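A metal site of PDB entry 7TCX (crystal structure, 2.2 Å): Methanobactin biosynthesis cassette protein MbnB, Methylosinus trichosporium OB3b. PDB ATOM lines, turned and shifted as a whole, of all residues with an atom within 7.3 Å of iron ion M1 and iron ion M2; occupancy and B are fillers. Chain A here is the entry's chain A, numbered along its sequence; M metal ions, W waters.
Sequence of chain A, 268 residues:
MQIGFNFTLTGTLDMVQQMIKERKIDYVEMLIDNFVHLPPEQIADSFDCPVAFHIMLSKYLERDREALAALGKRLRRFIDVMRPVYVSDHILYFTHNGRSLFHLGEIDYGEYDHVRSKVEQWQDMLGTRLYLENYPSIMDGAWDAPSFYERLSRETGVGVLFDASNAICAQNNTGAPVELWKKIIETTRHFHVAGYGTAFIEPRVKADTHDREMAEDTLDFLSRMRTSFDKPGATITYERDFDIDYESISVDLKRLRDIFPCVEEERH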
ATOM      1  N   GLU A  29      -0.451 -14.564  17.951  1.00  0.00           N
ATOM      2  CA  GLU A  29      -1.490 -13.701  17.406  1.00  0.00           C
ATOM      3  C   GLU A  29      -1.863 -14.222  16.015  1.00  0.00           C
ATOM      4  O   GLU A  29      -1.052 -14.154  15.086  1.00  0.00           O
ATOM      5  CB  GLU A  29      -1.032 -12.254  17.355  1.00  0.00           C
ATOM      6  CG  GLU A  29      -2.147 -11.244  17.127  1.00  0.00           C
ATOM      7  CD  GLU A  29      -1.617  -9.848  16.864  1.00  0.00           C
ATOM      8  OE1 GLU A  29      -1.329  -9.125  17.845  1.00  0.00           O
ATOM      9  OE2 GLU A  29      -1.472  -9.481  15.668  1.00  0.00           O
ATOM     10  N   LEU A  31      -3.648 -14.074  12.487  1.00  0.00           N
ATOM     11  CA  LEU A  31      -4.348 -13.303  11.458  1.00  0.00           C
ATOM     12  C   LEU A  31      -5.604 -14.091  11.097  1.00  0.00           C
ATOM     13  O   LEU A  31      -5.692 -14.766  10.067  1.00  0.00           O
ATOM     14  CB  LEU A  31      -3.451 -13.054  10.242  1.00  0.00           C
ATOM     15  CG  LEU A  31      -3.745 -11.779   9.467  1.00  0.00           C
ATOM     16  CD1 LEU A  31      -3.378 -10.538  10.307  1.00  0.00           C
ATOM     17  CD2 LEU A  31      -3.003 -11.742   8.124  1.00  0.00           C
ATOM     18  N   HIS A  54      -6.134 -11.011  15.195  1.00  0.00           N
ATOM     19  CA  HIS A  54      -5.905  -9.821  14.375  1.00  0.00           C
ATOM     20  C   HIS A  54      -6.669 -10.025  13.075  1.00  0.00           C
ATOM     21  O   HIS A  54      -6.492 -11.041  12.407  1.00  0.00           O
ATOM     22  CB  HIS A  54      -4.406  -9.641  14.118  1.00  0.00           C
ATOM     23  CG  HIS A  54      -4.003  -8.241  13.767  1.00  0.00           C
ATOM     24  ND1 HIS A  54      -4.408  -7.128  14.475  1.00  0.00           N
ATOM     25  CD2 HIS A  54      -3.163  -7.786  12.802  1.00  0.00           C
ATOM     26  CE1 HIS A  54      -3.872  -6.051  13.937  1.00  0.00           C
ATOM     27  NE2 HIS A  54      -3.106  -6.427  12.929  1.00  0.00           N
ATOM     28  N   ILE A  55      -7.549  -9.091  12.737  1.00  0.00           N
ATOM     29  CA  ILE A  55      -8.421  -9.191  11.565  1.00  0.00           C
ATOM     30  C   ILE A  55      -7.923  -8.202  10.510  1.00  0.00           C
ATOM     31  O   ILE A  55      -7.895  -6.993  10.756  1.00  0.00           O
ATOM     32  CB  ILE A  55      -9.882  -8.892  11.927  1.00  0.00           C
ATOM     33  CG1 ILE A  55     -10.407  -9.855  13.016  1.00  0.00           C
ATOM     34  CG2 ILE A  55     -10.748  -8.903  10.670  1.00  0.00           C
ATOM     35  CD1 ILE A  55     -11.478  -9.229  13.913  1.00  0.00           C
ATOM     36  N   MET A  56      -7.555  -8.721   9.333  1.00  0.00           N
ATOM     37  CA  MET A  56      -6.966  -7.886   8.286  1.00  0.00           C
ATOM     38  C   MET A  56      -7.991  -7.407   7.264  1.00  0.00           C
ATOM     39  O   MET A  56      -8.030  -6.210   6.931  1.00  0.00           O
ATOM     40  CB  MET A  56      -5.856  -8.646   7.565  1.00  0.00           C
ATOM     41  CG  MET A  56      -5.157  -7.837   6.446  1.00  0.00           C
ATOM     42  SD  MET A  56      -4.506  -6.216   6.976  1.00  0.00           S
ATOM     43  CE  MET A  56      -2.980  -6.785   7.699  1.00  0.00           C
ATOM     44  N   SER A  88      -8.618  -7.689  17.507  1.00  0.00           N
ATOM     45  CA  SER A  88      -8.152  -6.421  16.935  1.00  0.00           C
ATOM     46  C   SER A  88      -8.393  -6.367  15.432  1.00  0.00           C
ATOM     47  O   SER A  88      -8.519  -7.372  14.739  1.00  0.00           O
ATOM     48  CB  SER A  88      -6.667  -6.168  17.241  1.00  0.00           C
ATOM     49  OG  SER A  88      -5.863  -7.258  16.849  1.00  0.00           O
ATOM     50  N   ASP A  89      -8.474  -5.132  14.928  1.00  0.00           N
ATOM     51  CA  ASP A  89      -8.722  -4.874  13.521  1.00  0.00           C
ATOM     52  C   ASP A  89      -8.065  -3.537  13.182  1.00  0.00           C
ATOM     53  O   ASP A  89      -7.260  -3.010  13.962  1.00  0.00           O
ATOM     54  CB  ASP A  89     -10.235  -4.936  13.227  1.00  0.00           C
ATOM     55  CG  ASP A  89     -10.557  -5.193  11.744  1.00  0.00           C
ATOM     56  OD1 ASP A  89      -9.869  -4.662  10.813  1.00  0.00           O
ATOM     57  OD2 ASP A  89     -11.532  -5.934  11.503  1.00  0.00           O
ATOM     58  N   HIS A  90      -8.410  -2.972  12.027  1.00  0.00           N
ATOM     59  CA  HIS A  90      -7.655  -1.873  11.451  1.00  0.00           C
ATOM     60  C   HIS A  90      -8.560  -0.702  11.110  1.00  0.00           C
ATOM     61  O   HIS A  90      -9.786  -0.830  11.064  1.00  0.00           O
ATOM     62  CB  HIS A  90      -6.925  -2.311  10.179  1.00  0.00           C
ATOM     63  CG  HIS A  90      -5.861  -3.324  10.405  1.00  0.00           C
ATOM     64  ND1 HIS A  90      -6.136  -4.676  10.505  1.00  0.00           N
ATOM     65  CD2 HIS A  90      -4.521  -3.198  10.543  1.00  0.00           C
ATOM     66  CE1 HIS A  90      -5.002  -5.329  10.697  1.00  0.00           C
ATOM     67  NE2 HIS A  90      -4.005  -4.455  10.733  1.00  0.00           N
ATOM     68  N   LEU A  92      -8.418   1.216   7.824  1.00  0.00           N
ATOM     69  CA  LEU A  92      -7.748   1.246   6.538  1.00  0.00           C
ATOM     70  C   LEU A  92      -8.721   1.599   5.418  1.00  0.00           C
ATOM     71  O   LEU A  92      -9.925   1.324   5.494  1.00  0.00           O
ATOM     72  CB  LEU A  92      -7.086  -0.104   6.204  1.00  0.00           C
ATOM     73  CG  LEU A  92      -5.910  -0.467   7.084  1.00  0.00           C
ATOM     74  CD1 LEU A  92      -5.687  -1.943   6.994  1.00  0.00           C
ATOM     75  CD2 LEU A  92      -4.670   0.298   6.633  1.00  0.00           C
ATOM     76  N   GLU A 133      -5.908  -0.626  15.374  1.00  0.00           N
ATOM     77  CA  GLU A 133      -4.482  -0.370  15.254  1.00  0.00           C
ATOM     78  C   GLU A 133      -4.225   0.953  14.534  1.00  0.00           C
ATOM     79  O   GLU A 133      -4.975   1.351  13.644  1.00  0.00           O
ATOM     80  CB  GLU A 133      -3.829  -1.528  14.505  1.00  0.00           C
ATOM     81  CG  GLU A 133      -2.401  -1.276  14.048  1.00  0.00           C
ATOM     82  CD  GLU A 133      -1.712  -2.509  13.562  1.00  0.00           C
ATOM     83  OE1 GLU A 133      -2.396  -3.395  12.997  1.00  0.00           O
ATOM     84  OE2 GLU A 133      -0.495  -2.613  13.714  1.00  0.00           O
ATOM     85  N   ASN A 134      -3.145   1.648  14.944  1.00  0.00           N
ATOM     86  CA  ASN A 134      -2.695   2.862  14.243  1.00  0.00           C
ATOM     87  C   ASN A 134      -1.975   2.523  12.930  1.00  0.00           C
ATOM     88  O   ASN A 134      -1.345   1.486  12.797  1.00  0.00           O
ATOM     89  CB  ASN A 134      -1.738   3.688  15.111  1.00  0.00           C
ATOM     90  CG  ASN A 134      -0.588   2.849  15.660  1.00  0.00           C
ATOM     91  OD1 ASN A 134      -0.808   1.768  16.260  1.00  0.00           O
ATOM     92  ND2 ASN A 134       0.634   3.353  15.485  1.00  0.00           N
ATOM     93  N   LEU A 161      -4.835  -0.875  19.684  1.00  0.00           N
ATOM     94  CA  LEU A 161      -3.666  -1.734  19.567  1.00  0.00           C
ATOM     95  C   LEU A 161      -2.542  -0.838  19.058  1.00  0.00           C
ATOM     96  O   LEU A 161      -2.571  -0.405  17.902  1.00  0.00           O
ATOM     97  CB  LEU A 161      -3.916  -2.898  18.627  1.00  0.00           C
ATOM     98  CG  LEU A 161      -2.766  -3.880  18.368  1.00  0.00           C
ATOM     99  CD1 LEU A 161      -2.415  -4.691  19.600  1.00  0.00           C
ATOM    100  CD2 LEU A 161      -3.126  -4.806  17.226  1.00  0.00           C
ATOM    101  N   PHE A 162      -1.601  -0.497  19.928  1.00  0.00           N
ATOM    102  CA  PHE A 162      -0.610   0.501  19.564  1.00  0.00           C
ATOM    103  C   PHE A 162       0.580  -0.223  18.929  1.00  0.00           C
ATOM    104  O   PHE A 162       1.259  -1.033  19.581  1.00  0.00           O
ATOM    105  CB  PHE A 162      -0.194   1.353  20.751  1.00  0.00           C
ATOM    106  CG  PHE A 162       0.827   2.381  20.378  1.00  0.00           C
ATOM    107  CD1 PHE A 162       0.490   3.455  19.558  1.00  0.00           C
ATOM    108  CD2 PHE A 162       2.150   2.245  20.755  1.00  0.00           C
ATOM    109  CE1 PHE A 162       1.421   4.372  19.144  1.00  0.00           C
ATOM    110  CE2 PHE A 162       3.093   3.173  20.366  1.00  0.00           C
ATOM    111  CZ  PHE A 162       2.724   4.245  19.571  1.00  0.00           C
ATOM    112  N   ASP A 163       0.811   0.049  17.655  1.00  0.00           N
ATOM    113  CA  ASP A 163       1.944  -0.518  16.949  1.00  0.00           C
ATOM    114  C   ASP A 163       3.076   0.505  17.019  1.00  0.00           C
ATOM    115  O   ASP A 163       3.026   1.559  16.364  1.00  0.00           O
ATOM    116  CB  ASP A 163       1.569  -0.856  15.513  1.00  0.00           C
ATOM    117  CG  ASP A 163       2.688  -1.568  14.770  1.00  0.00           C
ATOM    118  OD1 ASP A 163       3.832  -1.078  14.815  1.00  0.00           O
ATOM    119  OD2 ASP A 163       2.432  -2.634  14.168  1.00  0.00           O
ATOM    120  N   ALA A 164       4.109   0.189  17.816  1.00  0.00           N
ATOM    121  CA  ALA A 164       5.187   1.144  18.064  1.00  0.00           C
ATOM    122  C   ALA A 164       5.989   1.446  16.792  1.00  0.00           C
ATOM    123  O   ALA A 164       6.440   2.576  16.572  1.00  0.00           O
ATOM    124  CB  ALA A 164       6.113   0.597  19.149  1.00  0.00           C
ATOM    125  N   SER A 165       6.200   0.438  15.944  1.00  0.00           N
ATOM    126  CA  SER A 165       7.025   0.744  14.783  1.00  0.00           C
ATOM    127  C   SER A 165       6.230   1.489  13.711  1.00  0.00           C
ATOM    128  O   SER A 165       6.819   2.299  12.985  1.00  0.00           O
ATOM    129  CB  SER A 165       7.679  -0.539  14.233  1.00  0.00           C
ATOM    130  OG  SER A 165       6.778  -1.593  13.943  1.00  0.00           O
ATOM    131  N   ASN A 166       4.912   1.268  13.599  1.00  0.00           N
ATOM    132  CA  ASN A 166       4.108   2.097  12.705  1.00  0.00           C
ATOM    133  C   ASN A 166       4.194   3.566  13.110  1.00  0.00           C
ATOM    134  O   ASN A 166       4.219   4.450  12.251  1.00  0.00           O
ATOM    135  CB  ASN A 166       2.649   1.684  12.702  1.00  0.00           C
ATOM    136  CG  ASN A 166       2.437   0.325  12.136  1.00  0.00           C
ATOM    137  OD1 ASN A 166       3.402  -0.354  11.808  1.00  0.00           O
ATOM    138  ND2 ASN A 166       1.180  -0.117  12.059  1.00  0.00           N
ATOM    139  N   PHE A 191       0.159  -4.300  22.293  1.00  0.00           N
ATOM    140  CA  PHE A 191       1.107  -3.602  21.448  1.00  0.00           C
ATOM    141  C   PHE A 191       1.567  -4.476  20.281  1.00  0.00           C
ATOM    142  O   PHE A 191       1.446  -5.703  20.308  1.00  0.00           O
ATOM    143  CB  PHE A 191       2.326  -3.136  22.255  1.00  0.00           C
ATOM    144  CG  PHE A 191       1.980  -2.117  23.307  1.00  0.00           C
ATOM    145  CD1 PHE A 191       1.756  -0.800  22.950  1.00  0.00           C
ATOM    146  CD2 PHE A 191       1.824  -2.492  24.637  1.00  0.00           C
ATOM    147  CE1 PHE A 191       1.413   0.146  23.926  1.00  0.00           C
ATOM    148  CE2 PHE A 191       1.460  -1.555  25.620  1.00  0.00           C
ATOM    149  CZ  PHE A 191       1.259  -0.233  25.269  1.00  0.00           C
ATOM    150  N   HIS A 192       2.071  -3.793  19.254  1.00  0.00           N
ATOM    151  CA  HIS A 192       2.768  -4.385  18.123  1.00  0.00           C
ATOM    152  C   HIS A 192       4.130  -3.727  17.960  1.00  0.00           C
ATOM    153  O   HIS A 192       4.343  -2.574  18.333  1.00  0.00           O
ATOM    154  CB  HIS A 192       2.040  -4.155  16.802  1.00  0.00           C
ATOM    155  CG  HIS A 192       1.015  -5.177  16.468  1.00  0.00           C
ATOM    156  ND1 HIS A 192       0.462  -5.280  15.216  1.00  0.00           N
ATOM    157  CD2 HIS A 192       0.403  -6.112  17.231  1.00  0.00           C
ATOM    158  CE1 HIS A 192      -0.427  -6.254  15.212  1.00  0.00           C
ATOM    159  NE2 HIS A 192      -0.479  -6.774  16.416  1.00  0.00           N
ATOM    160  N   VAL A 193       5.039  -4.477  17.339  1.00  0.00           N
ATOM    161  CA  VAL A 193       6.309  -3.920  16.899  1.00  0.00           C
ATOM    162  C   VAL A 193       6.855  -4.830  15.809  1.00  0.00           C
ATOM    163  O   VAL A 193       6.572  -6.042  15.798  1.00  0.00           O
ATOM    164  CB  VAL A 193       7.289  -3.769  18.092  1.00  0.00           C
ATOM    165  CG1 VAL A 193       7.783  -5.128  18.557  1.00  0.00           C
ATOM    166  CG2 VAL A 193       8.448  -2.889  17.687  1.00  0.00           C
ATOM    167  N   ALA A 194       7.598  -4.241  14.868  1.00  0.00           N
ATOM    168  CA  ALA A 194       8.182  -4.969  13.750  1.00  0.00           C
ATOM    169  C   ALA A 194       9.314  -4.140  13.144  1.00  0.00           C
ATOM    170  O   ALA A 194       9.564  -3.001  13.545  1.00  0.00           O
ATOM    171  CB  ALA A 194       7.136  -5.300  12.692  1.00  0.00           C
ATOM    172  N   ASP A 208       6.161   0.105   5.930  1.00  0.00           N
ATOM    173  CA  ASP A 208       5.817  -0.832   7.016  1.00  0.00           C
ATOM    174  C   ASP A 208       5.760  -2.252   6.473  1.00  0.00           C
ATOM    175  O   ASP A 208       4.698  -2.806   6.182  1.00  0.00           O
ATOM    176  CB  ASP A 208       4.493  -0.426   7.652  1.00  0.00           C
ATOM    177  CG  ASP A 208       4.223  -1.168   8.964  1.00  0.00           C
ATOM    178  OD1 ASP A 208       5.134  -1.218   9.816  1.00  0.00           O
ATOM    179  OD2 ASP A 208       3.089  -1.703   9.128  1.00  0.00           O
ATOM    180  N   HIS A 210       7.541  -5.258   7.712  1.00  0.00           N
ATOM    181  CA  HIS A 210       7.609  -6.415   8.623  1.00  0.00           C
ATOM    182  C   HIS A 210       8.515  -7.509   8.092  1.00  0.00           C
ATOM    183  O   HIS A 210       8.205  -8.691   8.169  1.00  0.00           O
ATOM    184  CB  HIS A 210       6.225  -7.019   8.895  1.00  0.00           C
ATOM    185  CG  HIS A 210       5.230  -6.027   9.387  1.00  0.00           C
ATOM    186  ND1 HIS A 210       3.908  -6.351   9.579  1.00  0.00           N
ATOM    187  CD2 HIS A 210       5.363  -4.730   9.747  1.00  0.00           C
ATOM    188  CE1 HIS A 210       3.258  -5.287  10.013  1.00  0.00           C
ATOM    189  NE2 HIS A 210       4.120  -4.287  10.118  1.00  0.00           N
ATOM    190  N   THR A 237       3.191  -7.984  20.374  1.00  0.00           N
ATOM    191  CA  THR A 237       3.374  -8.937  19.292  1.00  0.00           C
ATOM    192  C   THR A 237       4.496  -8.466  18.378  1.00  0.00           C
ATOM    193  O   THR A 237       4.452  -7.352  17.868  1.00  0.00           O
ATOM    194  CB  THR A 237       2.094  -9.097  18.479  1.00  0.00           C
ATOM    195  OG1 THR A 237       0.982  -9.341  19.339  1.00  0.00           O
ATOM    196  CG2 THR A 237       2.239 -10.233  17.462  1.00  0.00           C
ATOM    197  N   GLU A 239       5.982  -8.728  14.783  1.00  0.00           N
ATOM    198  CA  GLU A 239       5.438  -9.066  13.469  1.00  0.00           C
ATOM    199  C   GLU A 239       6.578  -9.352  12.495  1.00  0.00           C
ATOM    200  O   GLU A 239       7.502  -8.543  12.368  1.00  0.00           O
ATOM    201  CB  GLU A 239       4.563  -7.952  12.921  1.00  0.00           C
ATOM    202  CG  GLU A 239       3.517  -7.458  13.892  1.00  0.00           C
ATOM    203  CD  GLU A 239       2.555  -6.481  13.249  1.00  0.00           C
ATOM    204  OE1 GLU A 239       1.620  -6.904  12.538  1.00  0.00           O
ATOM    205  OE2 GLU A 239       2.759  -5.265  13.456  1.00  0.00           O
ATOM    206  N   ASP A 241       6.425 -10.770   8.551  1.00  0.00           N
ATOM    207  CA  ASP A 241       5.576 -11.264   7.480  1.00  0.00           C
ATOM    208  C   ASP A 241       6.359 -11.750   6.269  1.00  0.00           C
ATOM    209  O   ASP A 241       5.820 -12.484   5.447  1.00  0.00           O
ATOM    210  CB  ASP A 241       4.586 -10.171   7.056  1.00  0.00           C
ATOM    211  CG  ASP A 241       3.589  -9.813   8.173  1.00  0.00           C
ATOM    212  OD1 ASP A 241       3.213 -10.715   8.952  1.00  0.00           O
ATOM    213  OD2 ASP A 241       3.178  -8.645   8.287  1.00  0.00           O
HETATM  214 FE    FE M   1      -2.068  -4.942  11.507  1.00  0.00          FE
HETATM  215 FE    FE M   2       1.030  -3.937  13.320  1.00  0.00          FE
HETATM  216 FE    FE M   3       3.405  -2.443  11.178  1.00  0.00          FE
HETATM  217  O   HOH W   1      -1.080  -3.358   9.958  1.00  0.00           O
HETATM  218  O   HOH W   2      -1.541  -6.821  10.105  1.00  0.00           O
HETATM  219  O   HOH W   3      -0.277  -5.146  12.149  1.00  0.00           O
HETATM  220  O   HOH W   4       1.207  -2.992  11.083  1.00  0.00           O
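Within 4 Å of iron ion M1: His 54, His 90 and Glu 133.
The side-chain amide nitrogen of Asn 166 lies close to the side-chain carboxylate of Glu 133 (3.4 Å). The backbone NH (N) of Asn 166 lies within hydrogen-bond range of the side-chain carboxylate (OD1) of Asp 163 (2.9 Å). The backbone NH (N) of Asp 163 is in hydrogen-bond range of the side-chain amide oxygen (OD1) of Asn 134 (2.7 Å). N of Ser 165 is in hydrogen-bond range of OD1 of Asp 163 (3.0 Å). N of Glu 239 lies within hydrogen-bond range of O of Val 193 (2.9 Å). ND1 of His 54 is in hydrogen-bond range of OG of Ser 88 (2.8 Å). The backbone carbonyl oxygen of Phe 162 is in hydrogen-bond range of the backbone NH of His 192 (2.9 Å). O of His 192 sits at hydrogen-bond distance from N of Ala 164.
Four residues have an atom within 4 Å of iron ion M2: Glu 133, Asp 163, His 192 and Glu 239. The nearest printed residue that does not touch iron ion M2 is Asn 166 (4.03 Å).
OE2 of Glu 133 binds iron ion M2. Iron ion M2 is bound by OD2 of Asp 163 (2.1 Å). Water W3 binds iron ion M2 (2.1 Å). OE2 of Glu 239 binds iron ion M2, 2.2 Å away. ND1 of His 192 binds iron ion M2, at 2.4 Å. Water W4 binds iron ion M2 (2.4 Å). Iron ion M2 has six donor atoms within binding distance.
Iron ion M1 is bound by water W3 (1.9 Å), NE2 of His 90 (2.1 Å), OE1 of Glu 133 (2.2 Å), NE2 of His 54 (2.3 Å), water W2 (2.4 Å) and water W1 (2.4 Å).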
